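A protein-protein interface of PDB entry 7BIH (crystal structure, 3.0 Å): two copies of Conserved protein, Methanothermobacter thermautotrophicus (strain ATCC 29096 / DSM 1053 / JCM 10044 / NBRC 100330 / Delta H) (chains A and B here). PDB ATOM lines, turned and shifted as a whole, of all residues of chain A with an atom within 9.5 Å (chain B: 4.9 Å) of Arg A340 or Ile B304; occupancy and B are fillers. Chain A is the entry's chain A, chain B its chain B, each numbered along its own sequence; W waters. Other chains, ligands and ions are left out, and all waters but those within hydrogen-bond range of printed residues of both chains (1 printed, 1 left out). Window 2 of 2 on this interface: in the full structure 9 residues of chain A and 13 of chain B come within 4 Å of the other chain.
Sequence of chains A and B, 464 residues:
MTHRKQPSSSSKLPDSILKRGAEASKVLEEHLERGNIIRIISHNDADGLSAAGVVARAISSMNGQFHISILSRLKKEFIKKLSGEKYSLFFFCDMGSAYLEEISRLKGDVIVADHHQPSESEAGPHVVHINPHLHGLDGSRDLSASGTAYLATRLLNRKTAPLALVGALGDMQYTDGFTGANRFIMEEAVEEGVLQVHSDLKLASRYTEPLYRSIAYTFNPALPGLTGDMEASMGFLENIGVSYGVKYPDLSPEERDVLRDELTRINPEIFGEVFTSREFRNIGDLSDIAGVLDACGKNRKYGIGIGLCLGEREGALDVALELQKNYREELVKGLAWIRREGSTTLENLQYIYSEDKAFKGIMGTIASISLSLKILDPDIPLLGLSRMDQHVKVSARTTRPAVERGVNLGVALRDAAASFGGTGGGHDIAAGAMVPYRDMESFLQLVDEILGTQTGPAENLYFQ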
ATOM      1  N   VAL A 332     -10.378   5.981  23.190  1.00  0.00           N
ATOM      2  CA  VAL A 332     -10.205   4.556  22.866  1.00  0.00           C
ATOM      3  C   VAL A 332     -11.467   3.999  22.178  1.00  0.00           C
ATOM      4  O   VAL A 332     -11.351   3.309  21.161  1.00  0.00           O
ATOM      5  CB  VAL A 332      -9.836   3.711  24.112  1.00  0.00           C
ATOM      6  CG1 VAL A 332      -9.958   2.213  23.841  1.00  0.00           C
ATOM      7  CG2 VAL A 332      -8.416   4.034  24.550  1.00  0.00           C
ATOM      8  N   LYS A 333     -12.636   4.295  22.750  1.00  0.00           N
ATOM      9  CA  LYS A 333     -13.922   3.898  22.204  1.00  0.00           C
ATOM     10  C   LYS A 333     -14.155   4.476  20.820  1.00  0.00           C
ATOM     11  O   LYS A 333     -14.672   3.797  19.930  1.00  0.00           O
ATOM     12  CB  LYS A 333     -15.078   4.324  23.118  1.00  0.00           C
ATOM     13  CG  LYS A 333     -15.166   3.512  24.391  1.00  0.00           C
ATOM     14  CD  LYS A 333     -16.137   4.133  25.387  1.00  0.00           C
ATOM     15  CE  LYS A 333     -16.107   3.360  26.703  1.00  0.00           C
ATOM     16  NZ  LYS A 333     -16.885   4.049  27.763  1.00  0.00           N
ATOM     17  N   GLY A 334     -13.817   5.746  20.661  1.00  0.00           N
ATOM     18  CA  GLY A 334     -13.980   6.420  19.392  1.00  0.00           C
ATOM     19  C   GLY A 334     -13.139   5.760  18.312  1.00  0.00           C
ATOM     20  O   GLY A 334     -13.591   5.561  17.191  1.00  0.00           O
ATOM     21  N   LEU A 335     -11.913   5.422  18.663  1.00  0.00           N
ATOM     22  CA  LEU A 335     -11.042   4.720  17.741  1.00  0.00           C
ATOM     23  C   LEU A 335     -11.611   3.356  17.371  1.00  0.00           C
ATOM     24  O   LEU A 335     -11.576   2.943  16.197  1.00  0.00           O
ATOM     25  CB  LEU A 335      -9.640   4.596  18.334  1.00  0.00           C
ATOM     26  CG  LEU A 335      -8.796   5.832  18.049  1.00  0.00           C
ATOM     27  CD1 LEU A 335      -7.782   6.070  19.159  1.00  0.00           C
ATOM     28  CD2 LEU A 335      -8.110   5.639  16.714  1.00  0.00           C
ATOM     29  N   ALA A 336     -12.122   2.655  18.374  1.00  0.00           N
ATOM     30  CA  ALA A 336     -12.748   1.373  18.143  1.00  0.00           C
ATOM     31  C   ALA A 336     -13.925   1.534  17.180  1.00  0.00           C
ATOM     32  O   ALA A 336     -14.100   0.732  16.268  1.00  0.00           O
ATOM     33  CB  ALA A 336     -13.194   0.747  19.455  1.00  0.00           C
ATOM     34  N   TRP A 337     -14.719   2.569  17.381  1.00  0.00           N
ATOM     35  CA  TRP A 337     -15.853   2.826  16.513  1.00  0.00           C
ATOM     36  C   TRP A 337     -15.401   3.003  15.072  1.00  0.00           C
ATOM     37  O   TRP A 337     -15.969   2.381  14.177  1.00  0.00           O
ATOM     38  CB  TRP A 337     -16.679   4.018  17.012  1.00  0.00           C
ATOM     39  CG  TRP A 337     -17.685   4.511  16.037  1.00  0.00           C
ATOM     40  CD1 TRP A 337     -18.839   3.887  15.637  1.00  0.00           C
ATOM     41  CD2 TRP A 337     -17.634   5.749  15.336  1.00  0.00           C
ATOM     42  NE1 TRP A 337     -19.509   4.676  14.744  1.00  0.00           N
ATOM     43  CE2 TRP A 337     -18.790   5.823  14.527  1.00  0.00           C
ATOM     44  CE3 TRP A 337     -16.718   6.811  15.321  1.00  0.00           C
ATOM     45  CZ2 TRP A 337     -19.050   6.918  13.689  1.00  0.00           C
ATOM     46  CZ3 TRP A 337     -16.980   7.912  14.505  1.00  0.00           C
ATOM     47  CH2 TRP A 337     -18.135   7.957  13.704  1.00  0.00           C
ATOM     48  N   ILE A 338     -14.365   3.797  14.834  1.00  0.00           N
ATOM     49  CA  ILE A 338     -13.858   3.975  13.459  1.00  0.00           C
ATOM     50  C   ILE A 338     -13.393   2.633  12.890  1.00  0.00           C
ATOM     51  O   ILE A 338     -13.671   2.302  11.759  1.00  0.00           O
ATOM     52  CB  ILE A 338     -12.739   5.046  13.345  1.00  0.00           C
ATOM     53  CG1 ILE A 338     -13.295   6.432  13.702  1.00  0.00           C
ATOM     54  CG2 ILE A 338     -12.159   5.117  11.921  1.00  0.00           C
ATOM     55  CD1 ILE A 338     -12.244   7.520  13.840  1.00  0.00           C
ATOM     56  N   ARG A 339     -12.675   1.864  13.678  1.00  0.00           N
ATOM     57  CA  ARG A 339     -12.262   0.532  13.228  1.00  0.00           C
ATOM     58  C   ARG A 339     -13.479  -0.333  12.799  1.00  0.00           C
ATOM     59  O   ARG A 339     -13.445  -0.979  11.758  1.00  0.00           O
ATOM     60  CB  ARG A 339     -11.446  -0.173  14.294  1.00  0.00           C
ATOM     61  CG  ARG A 339     -10.004  -0.388  13.897  1.00  0.00           C
ATOM     62  CD  ARG A 339      -9.383  -1.308  14.885  1.00  0.00           C
ATOM     63  NE  ARG A 339      -8.507  -2.262  14.223  1.00  0.00           N
ATOM     64  CZ  ARG A 339      -7.715  -3.117  14.848  1.00  0.00           C
ATOM     65  NH1 ARG A 339      -6.977  -3.956  14.131  1.00  0.00           N
ATOM     66  NH2 ARG A 339      -7.630  -3.133  16.173  1.00  0.00           N
ATOM     67  N   ARG A 340     -14.540  -0.318  13.602  1.00  0.00           N
ATOM     68  CA  ARG A 340     -15.781  -1.054  13.323  1.00  0.00           C
ATOM     69  C   ARG A 340     -16.482  -0.533  12.063  1.00  0.00           C
ATOM     70  O   ARG A 340     -16.351  -1.161  11.028  1.00  0.00           O
ATOM     71  CB  ARG A 340     -16.695  -1.020  14.559  1.00  0.00           C
ATOM     72  CG  ARG A 340     -18.174  -1.404  14.397  1.00  0.00           C
ATOM     73  CD  ARG A 340     -18.924  -1.363  15.726  1.00  0.00           C
ATOM     74  NE  ARG A 340     -17.970  -1.329  16.851  1.00  0.00           N
ATOM     75  CZ  ARG A 340     -17.809  -0.339  17.741  1.00  0.00           C
ATOM     76  NH1 ARG A 340     -18.601   0.735  17.766  1.00  0.00           N
ATOM     77  NH2 ARG A 340     -16.856  -0.457  18.665  1.00  0.00           N
ATOM     78  N   GLU A 341     -17.236   0.571  12.143  1.00  0.00           N
ATOM     79  CA  GLU A 341     -17.800   1.224  10.945  1.00  0.00           C
ATOM     80  C   GLU A 341     -16.632   1.932  10.315  1.00  0.00           C
ATOM     81  O   GLU A 341     -15.919   2.630  11.015  1.00  0.00           O
ATOM     82  CB  GLU A 341     -18.860   2.273  11.293  1.00  0.00           C
ATOM     83  CG  GLU A 341     -19.935   1.812  12.252  1.00  0.00           C
ATOM     84  N   GLY A 342     -16.406   1.787   9.025  1.00  0.00           N
ATOM     85  CA  GLY A 342     -15.212   2.405   8.412  1.00  0.00           C
ATOM     86  C   GLY A 342     -15.559   3.811   7.988  1.00  0.00           C
ATOM     87  O   GLY A 342     -16.537   4.391   8.496  1.00  0.00           O
ATOM     88  N   SER A 343     -14.791   4.331   7.030  1.00  0.00           N
ATOM     89  CA  SER A 343     -15.157   5.554   6.326  1.00  0.00           C
ATOM     90  C   SER A 343     -15.577   5.260   4.876  1.00  0.00           C
ATOM     91  O   SER A 343     -15.091   4.299   4.295  1.00  0.00           O
ATOM     92  CB  SER A 343     -13.966   6.505   6.350  1.00  0.00           C
ATOM     93  OG  SER A 343     -12.897   6.088   5.507  1.00  0.00           O
ATOM     94  N   THR A 344     -16.467   6.067   4.295  1.00  0.00           N
ATOM     95  CA  THR A 344     -16.672   6.034   2.840  1.00  0.00           C
ATOM     96  C   THR A 344     -15.697   6.999   2.190  1.00  0.00           C
ATOM     97  O   THR A 344     -15.635   8.174   2.586  1.00  0.00           O
ATOM     98  CB  THR A 344     -18.116   6.342   2.409  1.00  0.00           C
ATOM     99  OG1 THR A 344     -18.572   7.505   3.049  1.00  0.00           O
ATOM    100  CG2 THR A 344     -19.049   5.266   2.855  1.00  0.00           C
ATOM    101  N   THR A 345     -14.952   6.491   1.208  1.00  0.00           N
ATOM    102  CA  THR A 345     -14.039   7.282   0.383  1.00  0.00           C
ATOM    103  C   THR A 345     -14.747   7.835  -0.866  1.00  0.00           C
ATOM    104  O   THR A 345     -15.559   7.170  -1.433  1.00  0.00           O
ATOM    105  CB  THR A 345     -12.884   6.373  -0.117  1.00  0.00           C
ATOM    106  OG1 THR A 345     -12.186   5.794   1.002  1.00  0.00           O
ATOM    107  CG2 THR A 345     -11.890   7.139  -0.966  1.00  0.00           C
ATOM    108  N   ILE A 352     -16.828  10.067   7.752  1.00  0.00           N
ATOM    109  CA  ILE A 352     -17.365   9.169   8.765  1.00  0.00           C
ATOM    110  C   ILE A 352     -18.544   9.939   9.410  1.00  0.00           C
ATOM    111  O   ILE A 352     -18.425  11.138   9.663  1.00  0.00           O
ATOM    112  CB  ILE A 352     -16.206   8.696   9.717  1.00  0.00           C
ATOM    113  CG1 ILE A 352     -16.548   7.500  10.644  1.00  0.00           C
ATOM    114  CG2 ILE A 352     -15.716   9.818  10.609  1.00  0.00           C
ATOM    115  CD1 ILE A 352     -17.767   6.631  10.311  1.00  0.00           C
ATOM    116  N   SER A 354     -21.785   9.927  12.402  1.00  0.00           N
ATOM    117  CA  SER A 354     -22.278   9.367  13.653  1.00  0.00           C
ATOM    118  C   SER A 354     -23.508  10.101  14.105  1.00  0.00           C
ATOM    119  O   SER A 354     -23.667  11.277  13.789  1.00  0.00           O
ATOM    120  CB  SER A 354     -21.239   9.525  14.738  1.00  0.00           C
ATOM    121  OG  SER A 354     -21.752   9.082  15.968  1.00  0.00           O
ATOM    122  N   ASP A 356     -24.077   9.525  17.559  1.00  0.00           N
ATOM    123  CA  ASP A 356     -23.736   9.478  18.991  1.00  0.00           C
ATOM    124  C   ASP A 356     -23.165  10.799  19.546  1.00  0.00           C
ATOM    125  O   ASP A 356     -22.394  11.492  18.889  1.00  0.00           O
ATOM    126  CB  ASP A 356     -22.739   8.353  19.264  1.00  0.00           C
ATOM    127  N   ALA A 358     -21.422  10.556  22.500  1.00  0.00           N
ATOM    128  CA  ALA A 358     -20.111  10.034  22.950  1.00  0.00           C
ATOM    129  C   ALA A 358     -18.903  10.611  22.201  1.00  0.00           C
ATOM    130  O   ALA A 358     -17.829  10.853  22.810  1.00  0.00           O
ATOM    131  CB  ALA A 358     -20.089   8.511  22.842  1.00  0.00           C
ATOM    132  N   PHE A 359     -19.090  10.819  20.892  1.00  0.00           N
ATOM    133  CA  PHE A 359     -18.019  11.247  20.000  1.00  0.00           C
ATOM    134  C   PHE A 359     -18.076  12.719  19.567  1.00  0.00           C
ATOM    135  O   PHE A 359     -17.111  13.193  18.988  1.00  0.00           O
ATOM    136  CB  PHE A 359     -17.983  10.337  18.762  1.00  0.00           C
ATOM    137  CG  PHE A 359     -18.046   8.861  19.097  1.00  0.00           C
ATOM    138  CD1 PHE A 359     -17.287   8.328  20.146  1.00  0.00           C
ATOM    139  CD2 PHE A 359     -18.866   7.999  18.375  1.00  0.00           C
ATOM    140  CE1 PHE A 359     -17.348   6.979  20.469  1.00  0.00           C
ATOM    141  CE2 PHE A 359     -18.934   6.646  18.695  1.00  0.00           C
ATOM    142  CZ  PHE A 359     -18.168   6.134  19.738  1.00  0.00           C
ATOM    143  N   ILE A 375      -5.412   3.454  10.233  1.00  0.00           N
ATOM    144  CA  ILE A 375      -6.734   2.822  10.164  1.00  0.00           C
ATOM    145  C   ILE A 375      -7.401   3.292   8.864  1.00  0.00           C
ATOM    146  O   ILE A 375      -8.084   2.524   8.156  1.00  0.00           O
ATOM    147  CB  ILE A 375      -7.664   3.246  11.335  1.00  0.00           C
ATOM    148  CG1 ILE A 375      -7.190   2.675  12.660  1.00  0.00           C
ATOM    149  CG2 ILE A 375      -9.110   2.768  11.122  1.00  0.00           C
ATOM    150  CD1 ILE A 375      -7.914   3.247  13.883  1.00  0.00           C
ATOM    151  N   LEU A 376      -7.214   4.580   8.585  1.00  0.00           N
ATOM    152  CA  LEU A 376      -7.721   5.208   7.405  1.00  0.00           C
ATOM    153  C   LEU A 376      -6.556   5.737   6.587  1.00  0.00           C
ATOM    154  O   LEU A 376      -5.509   6.059   7.138  1.00  0.00           O
ATOM    155  CB  LEU A 376      -8.672   6.324   7.822  1.00  0.00           C
ATOM    156  CG  LEU A 376      -9.887   5.862   8.641  1.00  0.00           C
ATOM    157  CD1 LEU A 376     -10.755   7.038   9.066  1.00  0.00           C
ATOM    158  CD2 LEU A 376     -10.770   4.862   7.891  1.00  0.00           C
ATOM    159  N   CYS B 296     -19.096  -3.846  -0.374  1.00  0.00           N
ATOM    160  CA  CYS B 296     -18.176  -2.896   0.264  1.00  0.00           C
ATOM    161  C   CYS B 296     -17.585  -1.885  -0.731  1.00  0.00           C
ATOM    162  O   CYS B 296     -17.447  -0.668  -0.460  1.00  0.00           O
ATOM    163  CB  CYS B 296     -17.024  -3.634   0.928  1.00  0.00           C
ATOM    164  SG  CYS B 296     -17.490  -4.580   2.394  1.00  0.00           S
ATOM    165  N   LYS B 301     -16.601   1.889   0.985  1.00  0.00           N
ATOM    166  CA  LYS B 301     -16.381   1.357   2.312  1.00  0.00           C
ATOM    167  C   LYS B 301     -15.186   0.390   2.128  1.00  0.00           C
ATOM    168  O   LYS B 301     -15.238  -0.772   2.505  1.00  0.00           O
ATOM    169  CB  LYS B 301     -17.655   0.659   2.736  1.00  0.00           C
ATOM    170  CG  LYS B 301     -18.099   0.968   4.137  1.00  0.00           C
ATOM    171  CD  LYS B 301     -18.656   2.361   4.304  1.00  0.00           C
ATOM    172  CE  LYS B 301     -19.095   2.511   5.753  1.00  0.00           C
ATOM    173  NZ  LYS B 301     -19.398   3.902   6.181  1.00  0.00           N
ATOM    174  N   TYR B 302     -14.090   0.936   1.582  1.00  0.00           N
ATOM    175  CA  TYR B 302     -12.924   0.152   1.231  1.00  0.00           C
ATOM    176  C   TYR B 302     -12.214  -0.447   2.432  1.00  0.00           C
ATOM    177  O   TYR B 302     -11.615  -1.547   2.382  1.00  0.00           O
ATOM    178  CB  TYR B 302     -11.945   1.038   0.478  1.00  0.00           C
ATOM    179  CG  TYR B 302     -12.491   1.721  -0.759  1.00  0.00           C
ATOM    180  CD1 TYR B 302     -13.427   1.088  -1.590  1.00  0.00           C
ATOM    181  CD2 TYR B 302     -12.016   2.963  -1.139  1.00  0.00           C
ATOM    182  CE1 TYR B 302     -13.894   1.698  -2.736  1.00  0.00           C
ATOM    183  CE2 TYR B 302     -12.476   3.574  -2.288  1.00  0.00           C
ATOM    184  CZ  TYR B 302     -13.419   2.941  -3.074  1.00  0.00           C
ATOM    185  OH  TYR B 302     -13.848   3.574  -4.210  1.00  0.00           O
ATOM    186  N   GLY B 303     -12.238   0.316   3.515  1.00  0.00           N
ATOM    187  CA  GLY B 303     -11.670  -0.171   4.778  1.00  0.00           C
ATOM    188  C   GLY B 303     -12.284  -1.428   5.327  1.00  0.00           C
ATOM    189  O   GLY B 303     -11.563  -2.290   5.811  1.00  0.00           O
ATOM    190  N   ILE B 304     -13.598  -1.518   5.265  1.00  0.00           N
ATOM    191  CA  ILE B 304     -14.280  -2.699   5.700  1.00  0.00           C
ATOM    192  C   ILE B 304     -13.838  -3.882   4.809  1.00  0.00           C
ATOM    193  O   ILE B 304     -13.414  -4.970   5.321  1.00  0.00           O
ATOM    194  CB  ILE B 304     -15.800  -2.544   5.609  1.00  0.00           C
ATOM    195  CG1 ILE B 304     -16.338  -1.377   6.481  1.00  0.00           C
ATOM    196  CG2 ILE B 304     -16.420  -3.870   5.941  1.00  0.00           C
ATOM    197  CD1 ILE B 304     -16.255  -1.573   7.967  1.00  0.00           C
ATOM    198  N   GLY B 305     -13.882  -3.688   3.490  1.00  0.00           N
ATOM    199  CA  GLY B 305     -13.470  -4.726   2.549  1.00  0.00           C
ATOM    200  C   GLY B 305     -12.095  -5.329   2.845  1.00  0.00           C
ATOM    201  O   GLY B 305     -11.935  -6.550   3.043  1.00  0.00           O
ATOM    202  N   ILE B 306     -11.110  -4.451   2.952  1.00  0.00           N
ATOM    203  CA  ILE B 306      -9.729  -4.875   3.212  1.00  0.00           C
ATOM    204  C   ILE B 306      -9.537  -5.467   4.614  1.00  0.00           C
ATOM    205  O   ILE B 306      -8.772  -6.419   4.783  1.00  0.00           O
ATOM    206  CB  ILE B 306      -8.740  -3.724   2.967  1.00  0.00           C
ATOM    207  CG1 ILE B 306      -8.735  -3.417   1.492  1.00  0.00           C
ATOM    208  CG2 ILE B 306      -7.319  -4.100   3.381  1.00  0.00           C
ATOM    209  CD1 ILE B 306      -8.017  -2.136   1.199  1.00  0.00           C
ATOM    210  N   GLY B 307     -10.218  -4.886   5.604  1.00  0.00           N
ATOM    211  CA  GLY B 307     -10.239  -5.427   6.954  1.00  0.00           C
ATOM    212  C   GLY B 307     -10.698  -6.860   6.952  1.00  0.00           C
ATOM    213  O   GLY B 307     -10.065  -7.730   7.555  1.00  0.00           O
ATOM    214  N   LEU B 308     -11.794  -7.098   6.236  1.00  0.00           N
ATOM    215  CA  LEU B 308     -12.316  -8.457   6.019  1.00  0.00           C
ATOM    216  C   LEU B 308     -11.249  -9.343   5.404  1.00  0.00           C
ATOM    217  O   LEU B 308     -10.987 -10.397   5.912  1.00  0.00           O
ATOM    218  CB  LEU B 308     -13.541  -8.453   5.115  1.00  0.00           C
ATOM    219  CG  LEU B 308     -14.717  -9.244   5.666  1.00  0.00           C
ATOM    220  CD1 LEU B 308     -15.448  -8.419   6.723  1.00  0.00           C
ATOM    221  CD2 LEU B 308     -15.684  -9.611   4.547  1.00  0.00           C
ATOM    222  N   GLY B 315     -17.007  -6.185  14.616  1.00  0.00           N
ATOM    223  CA  GLY B 315     -17.940  -5.121  14.272  1.00  0.00           C
ATOM    224  C   GLY B 315     -17.974  -4.926  12.768  1.00  0.00           C
ATOM    225  O   GLY B 315     -19.051  -4.729  12.179  1.00  0.00           O
ATOM    226  N   ALA B 316     -16.776  -5.002  12.165  1.00  0.00           N
ATOM    227  CA  ALA B 316     -16.578  -4.904  10.709  1.00  0.00           C
ATOM    228  C   ALA B 316     -17.492  -5.858   9.928  1.00  0.00           C
ATOM    229  O   ALA B 316     -18.183  -5.454   8.986  1.00  0.00           O
ATOM    230  CB  ALA B 316     -15.122  -5.175  10.367  1.00  0.00           C
ATOM    231  N   VAL B 319     -21.232  -4.818   9.978  1.00  0.00           N
ATOM    232  CA  VAL B 319     -21.344  -3.699   9.054  1.00  0.00           C
ATOM    233  C   VAL B 319     -21.343  -4.228   7.631  1.00  0.00           C
ATOM    234  O   VAL B 319     -22.166  -3.796   6.824  1.00  0.00           O
ATOM    235  CB  VAL B 319     -20.196  -2.670   9.248  1.00  0.00           C
ATOM    236  CG1 VAL B 319     -20.173  -1.633   8.124  1.00  0.00           C
ATOM    237  CG2 VAL B 319     -20.324  -1.943  10.578  1.00  0.00           C
ATOM    238  N   ALA B 320     -20.402  -5.136   7.335  1.00  0.00           N
ATOM    239  CA  ALA B 320     -20.272  -5.713   5.992  1.00  0.00           C
ATOM    240  C   ALA B 320     -21.536  -6.454   5.577  1.00  0.00           C
ATOM    241  O   ALA B 320     -22.069  -6.239   4.489  1.00  0.00           O
ATOM    242  CB  ALA B 320     -19.070  -6.632   5.909  1.00  0.00           C
HETATM  243  O   HOH W   1     -13.162   3.935   2.781  1.00  0.00           O
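No position is printed for both chains.
Water W1 lies within hydrogen-bond range of the backbone carbonyl oxygen (O) of Ser A343 (2.5 Å), the side-chain hydroxyl (OG1) of Thr A345 (2.8 Å) and the backbone NH (N) of Tyr B302 (3.4 Å).
N of Lys B301 sits at hydrogen-bond distance from O of Cys B296 (3.1 Å).
Ile B304 touches Arg A340 (CD1 to O, 3.1 Å).
Arg A340 touches Gly B315.
Arg A340 touches Ala B316 (O to CA, 3.8 Å).
Gly A342 touches Lys B301 (O to NZ, 3.7 Å).
Ile B304 touches Gly A342 (CD1 to N, 3.5 Å).
Ser A343 touches Lys B301.
Lys B301 touches Thr A344.
OG1 of Thr A345 touches CD2 of Tyr B302, 3.6 Å away.
Of the 21 printed residues of chain A, 5 touch a printed residue of chain B.
Along chain A the printed residues that touch a printed residue of chain B span positions 340 to 345.
Hydrophobic or aromatic side chains of chain B that line the printed part of chain A: Tyr B302 and Ile B304.
Among the printed residues, 8 pairs touch across the chains.
Arg A340 touches three residues of chain B.
Ile B304 touches just these residues of chain A: Arg A340 (3.1 Å) and Gly A342 (3.5 Å).
No residue of chain A comes within 4 Å of Gly B307.
Of the printed residues of chain A, Gly B315 touches Arg A340.
Of chain A, only Arg A340 (3.8 Å) comes within 4 Å of Ala B316.
Printed residues of chain A within 4 Å of Lys B301: Gly A342 (3.7 Å), Ser A343 (3.8 Å) and Thr A344 (3.3 Å).
Of the printed residues of chain A, Tyr B302 touches Thr A345.
Printed residues of chain B within 4 Å of Ser A343: Lys B301.
Ala A358 touches none of the printed residues of chain B.
The nearest printed residue of chain A that does not touch Lys B301 is Thr A345 (4.9 Å).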
